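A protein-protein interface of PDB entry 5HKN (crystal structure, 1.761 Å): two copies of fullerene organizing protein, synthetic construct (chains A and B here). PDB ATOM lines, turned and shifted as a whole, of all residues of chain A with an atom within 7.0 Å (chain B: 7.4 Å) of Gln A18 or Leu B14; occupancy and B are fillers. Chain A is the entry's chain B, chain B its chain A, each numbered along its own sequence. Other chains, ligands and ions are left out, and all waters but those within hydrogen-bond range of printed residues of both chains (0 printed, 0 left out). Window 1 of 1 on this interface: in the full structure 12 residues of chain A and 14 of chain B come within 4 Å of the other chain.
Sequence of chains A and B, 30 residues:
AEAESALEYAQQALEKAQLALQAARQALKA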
ATOM      1  N   GLN A  11     -26.485  29.474  -9.366  1.00  0.00           N
ATOM      2  CA  GLN A  11     -25.308  29.256  -8.522  1.00  0.00           C
ATOM      3  C   GLN A  11     -25.246  27.797  -8.036  1.00  0.00           C
ATOM      4  O   GLN A  11     -24.185  27.168  -8.096  1.00  0.00           O
ATOM      5  CB  GLN A  11     -25.294  30.229  -7.342  1.00  0.00           C
ATOM      6  CG  GLN A  11     -23.916  30.396  -6.697  1.00  0.00           C
ATOM      7  CD  GLN A  11     -23.201  31.685  -7.124  1.00  0.00           C
ATOM      8  OE1 GLN A  11     -23.660  32.790  -6.824  1.00  0.00           O
ATOM      9  NE2 GLN A  11     -22.076  31.545  -7.822  1.00  0.00           N
ATOM     10  N   GLN A  12     -26.376  27.255  -7.589  1.00  0.00           N
ATOM     11  CA  GLN A  12     -26.437  25.864  -7.146  1.00  0.00           C
ATOM     12  C   GLN A  12     -26.056  24.906  -8.284  1.00  0.00           C
ATOM     13  O   GLN A  12     -25.301  23.973  -8.081  1.00  0.00           O
ATOM     14  CB  GLN A  12     -27.829  25.537  -6.611  1.00  0.00           C
ATOM     15  CG  GLN A  12     -28.160  26.267  -5.328  1.00  0.00           C
ATOM     16  CD  GLN A  12     -29.646  26.247  -5.008  1.00  0.00           C
ATOM     17  OE1 GLN A  12     -30.455  25.755  -5.797  1.00  0.00           O
ATOM     18  NE2 GLN A  12     -30.012  26.788  -3.849  1.00  0.00           N
ATOM     19  N   ALA A  13     -26.559  25.173  -9.487  1.00  0.00           N
ATOM     20  CA  ALA A  13     -26.237  24.358 -10.654  1.00  0.00           C
ATOM     21  C   ALA A  13     -24.742  24.422 -10.985  1.00  0.00           C
ATOM     22  O   ALA A  13     -24.143  23.412 -11.342  1.00  0.00           O
ATOM     23  CB  ALA A  13     -27.072  24.809 -11.863  1.00  0.00           C
ATOM     24  N   LEU A  14     -24.150  25.603 -10.868  1.00  0.00           N
ATOM     25  CA  LEU A  14     -22.725  25.769 -11.115  1.00  0.00           C
ATOM     26  C   LEU A  14     -21.909  24.994 -10.075  1.00  0.00           C
ATOM     27  O   LEU A  14     -20.890  24.392 -10.415  1.00  0.00           O
ATOM     28  CB  LEU A  14     -22.326  27.241 -11.097  1.00  0.00           C
ATOM     29  CG  LEU A  14     -22.860  28.116 -12.229  1.00  0.00           C
ATOM     30  CD1 LEU A  14     -22.137  29.460 -12.235  1.00  0.00           C
ATOM     31  CD2 LEU A  14     -22.691  27.404 -13.560  1.00  0.00           C
ATOM     32  N   GLU A  15     -22.359  25.021  -8.819  1.00  0.00           N
ATOM     33  CA  GLU A  15     -21.703  24.254  -7.751  1.00  0.00           C
ATOM     34  C   GLU A  15     -21.718  22.763  -8.072  1.00  0.00           C
ATOM     35  O   GLU A  15     -20.710  22.060  -7.862  1.00  0.00           O
ATOM     36  CB  GLU A  15     -22.363  24.527  -6.397  1.00  0.00           C
ATOM     37  CG  GLU A  15     -22.098  25.942  -5.863  1.00  0.00           C
ATOM     38  CD  GLU A  15     -22.968  26.307  -4.675  1.00  0.00           C
ATOM     39  OE1 GLU A  15     -23.821  25.479  -4.274  1.00  0.00           O
ATOM     40  OE2 GLU A  15     -22.794  27.429  -4.140  1.00  0.00           O
ATOM     41  N   LYS A  16     -22.836  22.271  -8.601  1.00  0.00           N
ATOM     42  CA  LYS A  16     -22.921  20.861  -8.970  1.00  0.00           C
ATOM     43  C   LYS A  16     -21.995  20.537 -10.140  1.00  0.00           C
ATOM     44  O   LYS A  16     -21.330  19.500 -10.139  1.00  0.00           O
ATOM     45  CB  LYS A  16     -24.362  20.468  -9.298  1.00  0.00           C
ATOM     46  CG  LYS A  16     -25.271  20.498  -8.094  1.00  0.00           C
ATOM     47  CD  LYS A  16     -26.705  20.142  -8.461  1.00  0.00           C
ATOM     48  CE  LYS A  16     -27.582  20.165  -7.221  1.00  0.00           C
ATOM     49  NZ  LYS A  16     -29.009  19.942  -7.567  1.00  0.00           N
ATOM     50  N   ALA A  17     -21.938  21.426 -11.133  1.00  0.00           N
ATOM     51  CA  ALA A  17     -21.026  21.238 -12.251  1.00  0.00           C
ATOM     52  C   ALA A  17     -19.581  21.169 -11.746  1.00  0.00           C
ATOM     53  O   ALA A  17     -18.803  20.329 -12.184  1.00  0.00           O
ATOM     54  CB  ALA A  17     -21.189  22.364 -13.273  1.00  0.00           C
ATOM     55  N   GLN A  18     -19.238  22.041 -10.804  1.00  0.00           N
ATOM     56  CA  GLN A  18     -17.868  22.127 -10.309  1.00  0.00           C
ATOM     57  C   GLN A  18     -17.461  20.847  -9.597  1.00  0.00           C
ATOM     58  O   GLN A  18     -16.334  20.366  -9.743  1.00  0.00           O
ATOM     59  CB  GLN A  18     -17.717  23.322  -9.368  1.00  0.00           C
ATOM     60  CG  GLN A  18     -17.688  24.657 -10.087  1.00  0.00           C
ATOM     61  CD  GLN A  18     -16.292  25.261 -10.149  1.00  0.00           C
ATOM     62  OE1 GLN A  18     -15.366  24.696 -10.751  1.00  0.00           O
ATOM     63  NE2 GLN A  18     -16.128  26.404  -9.495  1.00  0.00           N
ATOM     64  N   LEU A  19     -18.367  20.299  -8.803  1.00  0.00           N
ATOM     65  CA  LEU A  19     -17.990  19.117  -8.034  1.00  0.00           C
ATOM     66  C   LEU A  19     -17.873  17.896  -8.944  1.00  0.00           C
ATOM     67  O   LEU A  19     -17.028  17.029  -8.724  1.00  0.00           O
ATOM     68  CB  LEU A  19     -18.978  18.878  -6.887  1.00  0.00           C
ATOM     69  CG  LEU A  19     -20.439  18.492  -7.143  1.00  0.00           C
ATOM     70  CD1 LEU A  19     -20.571  16.984  -7.297  1.00  0.00           C
ATOM     71  CD2 LEU A  19     -21.326  18.971  -6.007  1.00  0.00           C
ATOM     72  N   ALA A  20     -18.706  17.822  -9.979  1.00  0.00           N
ATOM     73  CA  ALA A  20     -18.597  16.738 -10.947  1.00  0.00           C
ATOM     74  C   ALA A  20     -17.296  16.872 -11.743  1.00  0.00           C
ATOM     75  O   ALA A  20     -16.601  15.886 -12.021  1.00  0.00           O
ATOM     76  CB  ALA A  20     -19.807  16.734 -11.894  1.00  0.00           C
ATOM     77  N   LEU A  21     -16.970  18.105 -12.116  1.00  0.00           N
ATOM     78  CA  LEU A  21     -15.735  18.376 -12.848  1.00  0.00           C
ATOM     79  C   LEU A  21     -14.517  17.899 -12.046  1.00  0.00           C
ATOM     80  O   LEU A  21     -13.584  17.313 -12.597  1.00  0.00           O
ATOM     81  CB  LEU A  21     -15.642  19.878 -13.155  1.00  0.00           C
ATOM     82  CG  LEU A  21     -14.568  20.501 -14.040  1.00  0.00           C
ATOM     83  CD1 LEU A  21     -14.320  19.693 -15.298  1.00  0.00           C
ATOM     84  CD2 LEU A  21     -15.049  21.918 -14.406  1.00  0.00           C
ATOM     85  N   GLN A  22     -14.545  18.117 -10.737  1.00  0.00           N
ATOM     86  CA  GLN A  22     -13.438  17.695  -9.883  1.00  0.00           C
ATOM     87  C   GLN A  22     -13.316  16.178  -9.837  1.00  0.00           C
ATOM     88  O   GLN A  22     -12.205  15.644  -9.861  1.00  0.00           O
ATOM     89  CB  GLN A  22     -13.599  18.257  -8.473  1.00  0.00           C
ATOM     90  CG  GLN A  22     -13.164  19.715  -8.356  1.00  0.00           C
ATOM     91  CD  GLN A  22     -11.659  19.860  -8.501  1.00  0.00           C
ATOM     92  OE1 GLN A  22     -11.156  20.154  -9.577  1.00  0.00           O
ATOM     93  NE2 GLN A  22     -10.933  19.629  -7.409  1.00  0.00           N
ATOM     94  N   ALA A  23     -14.451  15.484  -9.787  1.00  0.00           N
ATOM     95  CA  ALA A  23     -14.436  14.025  -9.867  1.00  0.00           C
ATOM     96  C   ALA A  23     -13.818  13.588 -11.193  1.00  0.00           C
ATOM     97  O   ALA A  23     -12.958  12.709 -11.224  1.00  0.00           O
ATOM     98  CB  ALA A  23     -15.839  13.461  -9.713  1.00  0.00           C
ATOM     99  N   ALA A  24     -14.238  14.226 -12.287  1.00  0.00           N
ATOM    100  CA  ALA A  24     -13.717  13.890 -13.611  1.00  0.00           C
ATOM    101  C   ALA A  24     -12.214  14.111 -13.696  1.00  0.00           C
ATOM    102  O   ALA A  24     -11.496  13.276 -14.232  1.00  0.00           O
ATOM    103  CB  ALA A  24     -14.429  14.699 -14.688  1.00  0.00           C
ATOM    104  N   LEU B   7     -10.487  20.370 -19.061  1.00  0.00           N
ATOM    105  CA  LEU B   7     -11.185  20.383 -17.780  1.00  0.00           C
ATOM    106  C   LEU B   7     -10.646  21.460 -16.858  1.00  0.00           C
ATOM    107  O   LEU B   7     -11.402  22.079 -16.111  1.00  0.00           O
ATOM    108  CB  LEU B   7     -11.092  19.017 -17.095  1.00  0.00           C
ATOM    109  CG  LEU B   7     -11.788  17.863 -17.816  1.00  0.00           C
ATOM    110  CD1 LEU B   7     -11.874  16.654 -16.895  1.00  0.00           C
ATOM    111  CD2 LEU B   7     -13.165  18.270 -18.322  1.00  0.00           C
ATOM    112  N   GLU B   8      -9.339  21.683 -16.899  1.00  0.00           N
ATOM    113  CA  GLU B   8      -8.734  22.740 -16.093  1.00  0.00           C
ATOM    114  C   GLU B   8      -9.243  24.109 -16.554  1.00  0.00           C
ATOM    115  O   GLU B   8      -9.584  24.979 -15.745  1.00  0.00           O
ATOM    116  CB  GLU B   8      -7.212  22.667 -16.195  1.00  0.00           C
ATOM    117  CG  GLU B   8      -6.464  23.326 -15.057  1.00  0.00           C
ATOM    118  CD  GLU B   8      -4.960  23.166 -15.196  1.00  0.00           C
ATOM    119  OE1 GLU B   8      -4.524  22.157 -15.805  1.00  0.00           O
ATOM    120  OE2 GLU B   8      -4.221  24.044 -14.698  1.00  0.00           O
ATOM    121  N   TYR B   9      -9.334  24.278 -17.868  1.00  0.00           N
ATOM    122  CA  TYR B   9      -9.871  25.507 -18.439  1.00  0.00           C
ATOM    123  C   TYR B   9     -11.339  25.694 -18.070  1.00  0.00           C
ATOM    124  O   TYR B   9     -11.749  26.795 -17.719  1.00  0.00           O
ATOM    125  CB  TYR B   9      -9.691  25.493 -19.949  1.00  0.00           C
ATOM    126  CG  TYR B   9     -10.314  26.634 -20.718  1.00  0.00           C
ATOM    127  CD1 TYR B   9     -11.620  26.543 -21.182  1.00  0.00           C
ATOM    128  CD2 TYR B   9      -9.587  27.779 -21.030  1.00  0.00           C
ATOM    129  CE1 TYR B   9     -12.191  27.551 -21.916  1.00  0.00           C
ATOM    130  CE2 TYR B   9     -10.157  28.809 -21.775  1.00  0.00           C
ATOM    131  CZ  TYR B   9     -11.459  28.683 -22.211  1.00  0.00           C
ATOM    132  OH  TYR B   9     -12.053  29.682 -22.942  1.00  0.00           O
ATOM    133  N   ALA B  10     -12.126  24.621 -18.155  1.00  0.00           N
ATOM    134  CA  ALA B  10     -13.548  24.702 -17.838  1.00  0.00           C
ATOM    135  C   ALA B  10     -13.741  25.079 -16.374  1.00  0.00           C
ATOM    136  O   ALA B  10     -14.621  25.891 -16.042  1.00  0.00           O
ATOM    137  CB  ALA B  10     -14.255  23.378 -18.156  1.00  0.00           C
ATOM    138  N   GLN B  11     -12.923  24.498 -15.503  1.00  0.00           N
ATOM    139  CA  GLN B  11     -12.993  24.834 -14.077  1.00  0.00           C
ATOM    140  C   GLN B  11     -12.730  26.325 -13.848  1.00  0.00           C
ATOM    141  O   GLN B  11     -13.465  26.975 -13.111  1.00  0.00           O
ATOM    142  CB  GLN B  11     -12.015  23.976 -13.271  1.00  0.00           C
ATOM    143  CG  GLN B  11     -12.073  24.202 -11.769  1.00  0.00           C
ATOM    144  CD  GLN B  11     -11.037  23.381 -11.003  1.00  0.00           C
ATOM    145  OE1 GLN B  11     -10.428  22.460 -11.551  1.00  0.00           O
ATOM    146  NE2 GLN B  11     -10.833  23.718  -9.727  1.00  0.00           N
ATOM    147  N   GLN B  12     -11.713  26.866 -14.508  1.00  0.00           N
ATOM    148  CA  GLN B  12     -11.367  28.274 -14.358  1.00  0.00           C
ATOM    149  C   GLN B  12     -12.495  29.167 -14.865  1.00  0.00           C
ATOM    150  O   GLN B  12     -12.835  30.148 -14.229  1.00  0.00           O
ATOM    151  CB  GLN B  12     -10.057  28.577 -15.085  1.00  0.00           C
ATOM    152  CG  GLN B  12      -8.877  27.856 -14.471  1.00  0.00           C
ATOM    153  CD  GLN B  12      -7.636  27.868 -15.344  1.00  0.00           C
ATOM    154  OE1 GLN B  12      -7.653  28.363 -16.470  1.00  0.00           O
ATOM    155  NE2 GLN B  12      -6.552  27.298 -14.829  1.00  0.00           N
ATOM    156  N   ALA B  13     -13.089  28.795 -15.999  1.00  0.00           N
ATOM    157  CA  ALA B  13     -14.234  29.521 -16.549  1.00  0.00           C
ATOM    158  C   ALA B  13     -15.417  29.500 -15.596  1.00  0.00           C
ATOM    159  O   ALA B  13     -16.061  30.524 -15.388  1.00  0.00           O
ATOM    160  CB  ALA B  13     -14.637  28.939 -17.912  1.00  0.00           C
ATOM    161  N   LEU B  14     -15.704  28.345 -15.010  1.00  0.00           N
ATOM    162  CA  LEU B  14     -16.785  28.238 -14.037  1.00  0.00           C
ATOM    163  C   LEU B  14     -16.510  29.115 -12.818  1.00  0.00           C
ATOM    164  O   LEU B  14     -17.433  29.730 -12.281  1.00  0.00           O
ATOM    165  CB  LEU B  14     -16.987  26.789 -13.592  1.00  0.00           C
ATOM    166  CG  LEU B  14     -17.492  25.830 -14.670  1.00  0.00           C
ATOM    167  CD1 LEU B  14     -17.873  24.485 -14.053  1.00  0.00           C
ATOM    168  CD2 LEU B  14     -18.674  26.463 -15.361  1.00  0.00           C
ATOM    169  N   GLU B  15     -15.244  29.177 -12.394  1.00  0.00           N
ATOM    170  CA  GLU B  15     -14.871  30.024 -11.261  1.00  0.00           C
ATOM    171  C   GLU B  15     -15.176  31.483 -11.579  1.00  0.00           C
ATOM    172  O   GLU B  15     -15.719  32.215 -10.745  1.00  0.00           O
ATOM    173  CB  GLU B  15     -13.394  29.846 -10.904  1.00  0.00           C
ATOM    174  CG  GLU B  15     -13.124  28.612 -10.061  1.00  0.00           C
ATOM    175  CD  GLU B  15     -11.653  28.246 -10.004  1.00  0.00           C
ATOM    176  OE1 GLU B  15     -10.820  29.020 -10.532  1.00  0.00           O
ATOM    177  OE2 GLU B  15     -11.329  27.191  -9.413  1.00  0.00           O
ATOM    178  N   LYS B  16     -14.861  31.897 -12.795  1.00  0.00           N
ATOM    179  CA  LYS B  16     -15.147  33.260 -13.212  1.00  0.00           C
ATOM    180  C   LYS B  16     -16.654  33.512 -13.241  1.00  0.00           C
ATOM    181  O   LYS B  16     -17.125  34.553 -12.774  1.00  0.00           O
ATOM    182  CB  LYS B  16     -14.512  33.543 -14.570  1.00  0.00           C
ATOM    183  CG  LYS B  16     -13.010  33.443 -14.536  1.00  0.00           C
ATOM    184  CD  LYS B  16     -12.379  33.810 -15.867  1.00  0.00           C
ATOM    185  CE  LYS B  16     -10.868  33.770 -15.725  1.00  0.00           C
ATOM    186  NZ  LYS B  16     -10.187  34.104 -16.993  1.00  0.00           N
ATOM    187  N   ALA B  17     -17.421  32.552 -13.756  1.00  0.00           N
ATOM    188  CA  ALA B  17     -18.866  32.715 -13.798  1.00  0.00           C
ATOM    189  C   ALA B  17     -19.423  32.864 -12.380  1.00  0.00           C
ATOM    190  O   ALA B  17     -20.301  33.683 -12.132  1.00  0.00           O
ATOM    191  CB  ALA B  17     -19.521  31.546 -14.509  1.00  0.00           C
ATOM    192  N   GLN B  18     -18.883  32.084 -11.448  1.00  0.00           N
ATOM    193  CA  GLN B  18     -19.372  32.085 -10.074  1.00  0.00           C
ATOM    194  C   GLN B  18     -19.151  33.434  -9.403  1.00  0.00           C
ATOM    195  O   GLN B  18     -20.005  33.926  -8.678  1.00  0.00           O
ATOM    196  CB  GLN B  18     -18.684  30.987  -9.258  1.00  0.00           C
ATOM    197  CG  GLN B  18     -19.176  29.577  -9.571  1.00  0.00           C
ATOM    198  CD  GLN B  18     -20.052  28.987  -8.471  1.00  0.00           C
ATOM    199  OE1 GLN B  18     -21.090  29.551  -8.094  1.00  0.00           O
ATOM    200  NE2 GLN B  18     -19.624  27.847  -7.939  1.00  0.00           N
ATOM    201  N   LEU B  19     -17.988  34.024  -9.636  1.00  0.00           N
ATOM    202  CA  LEU B  19     -17.665  35.259  -8.946  1.00  0.00           C
ATOM    203  C   LEU B  19     -18.484  36.411  -9.515  1.00  0.00           C
ATOM    204  O   LEU B  19     -18.896  37.302  -8.778  1.00  0.00           O
ATOM    205  CB  LEU B  19     -16.159  35.530  -9.015  1.00  0.00           C
ATOM    206  CG  LEU B  19     -15.417  35.866 -10.310  1.00  0.00           C
ATOM    207  CD1 LEU B  19     -15.485  37.370 -10.559  1.00  0.00           C
ATOM    208  CD2 LEU B  19     -13.966  35.432 -10.231  1.00  0.00           C
ATOM    209  N   ALA B  20     -18.746  36.387 -10.822  1.00  0.00           N
ATOM    210  CA  ALA B  20     -19.603  37.395 -11.429  1.00  0.00           C
ATOM    211  C   ALA B  20     -21.045  37.238 -10.937  1.00  0.00           C
ATOM    212  O   ALA B  20     -21.729  38.226 -10.672  1.00  0.00           O
ATOM    213  CB  ALA B  20     -19.543  37.308 -12.956  1.00  0.00           C
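Gln A11 touches Gln B18, and with the chains exchanged Gln A18 touches Gln B11.
Leu A14 touches Gln B18, and with the chains exchanged Gln A18 touches Leu B14.
Glu A15 touches Gln B18, and with the chains exchanged Gln A18 touches Glu B15.
Of the 12 pairs that touch across the chains among the printed residues, 6 have their exchanged pair printed and touching as well.
Of chain B, only Gln B11 (3.5 Å), Leu B14 (3.8 Å) and Glu B15 (3.8 Å) come within 4 Å of Gln A18.
Of the printed residues of chain B, Leu A21 touches Leu B7 (3.5 Å), Ala B10 (3.9 Å), Gln B11 (3.5 Å) and Leu B14 (3.8 Å).
Glu B8 touches none of the printed residues of chain A.
Printed residues of chain A within 4 Å of Leu B14: Gln A18 and Leu A21.
Printed residues of chain A within 4 Å of Gln B18: Gln A11 (2.2 Å), Leu A14 (3.9 Å) and Glu A15 (3.7 Å).
Among the printed residues, pairs that only touch across the chains: Gln A18 with Gln B11, Leu A21 with Gln B11, Leu A21 with Leu B7, Glu A15 with Gln B18, Gln A18 with Glu B15, Gln A18 with Leu B14, Leu A21 with Leu B14, Leu A14 with Gln B18, Ala A24 with Leu B7 and Leu A21 with Ala B10.
OE1 of Gln B11 lies close to OE1 of Gln A22.
The backbone carbonyl oxygen of Gln B18 lies within hydrogen-bond range of the side-chain amide nitrogen of Gln A11 (3.3 Å).
Hydrophobic or aromatic side chains of chain B that line the printed part of chain A: Leu B7 and Leu B14.
Hydrophobic or aromatic side chains of chain A that line the printed part of chain B: Leu A14, Leu A21 and Ala A24.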
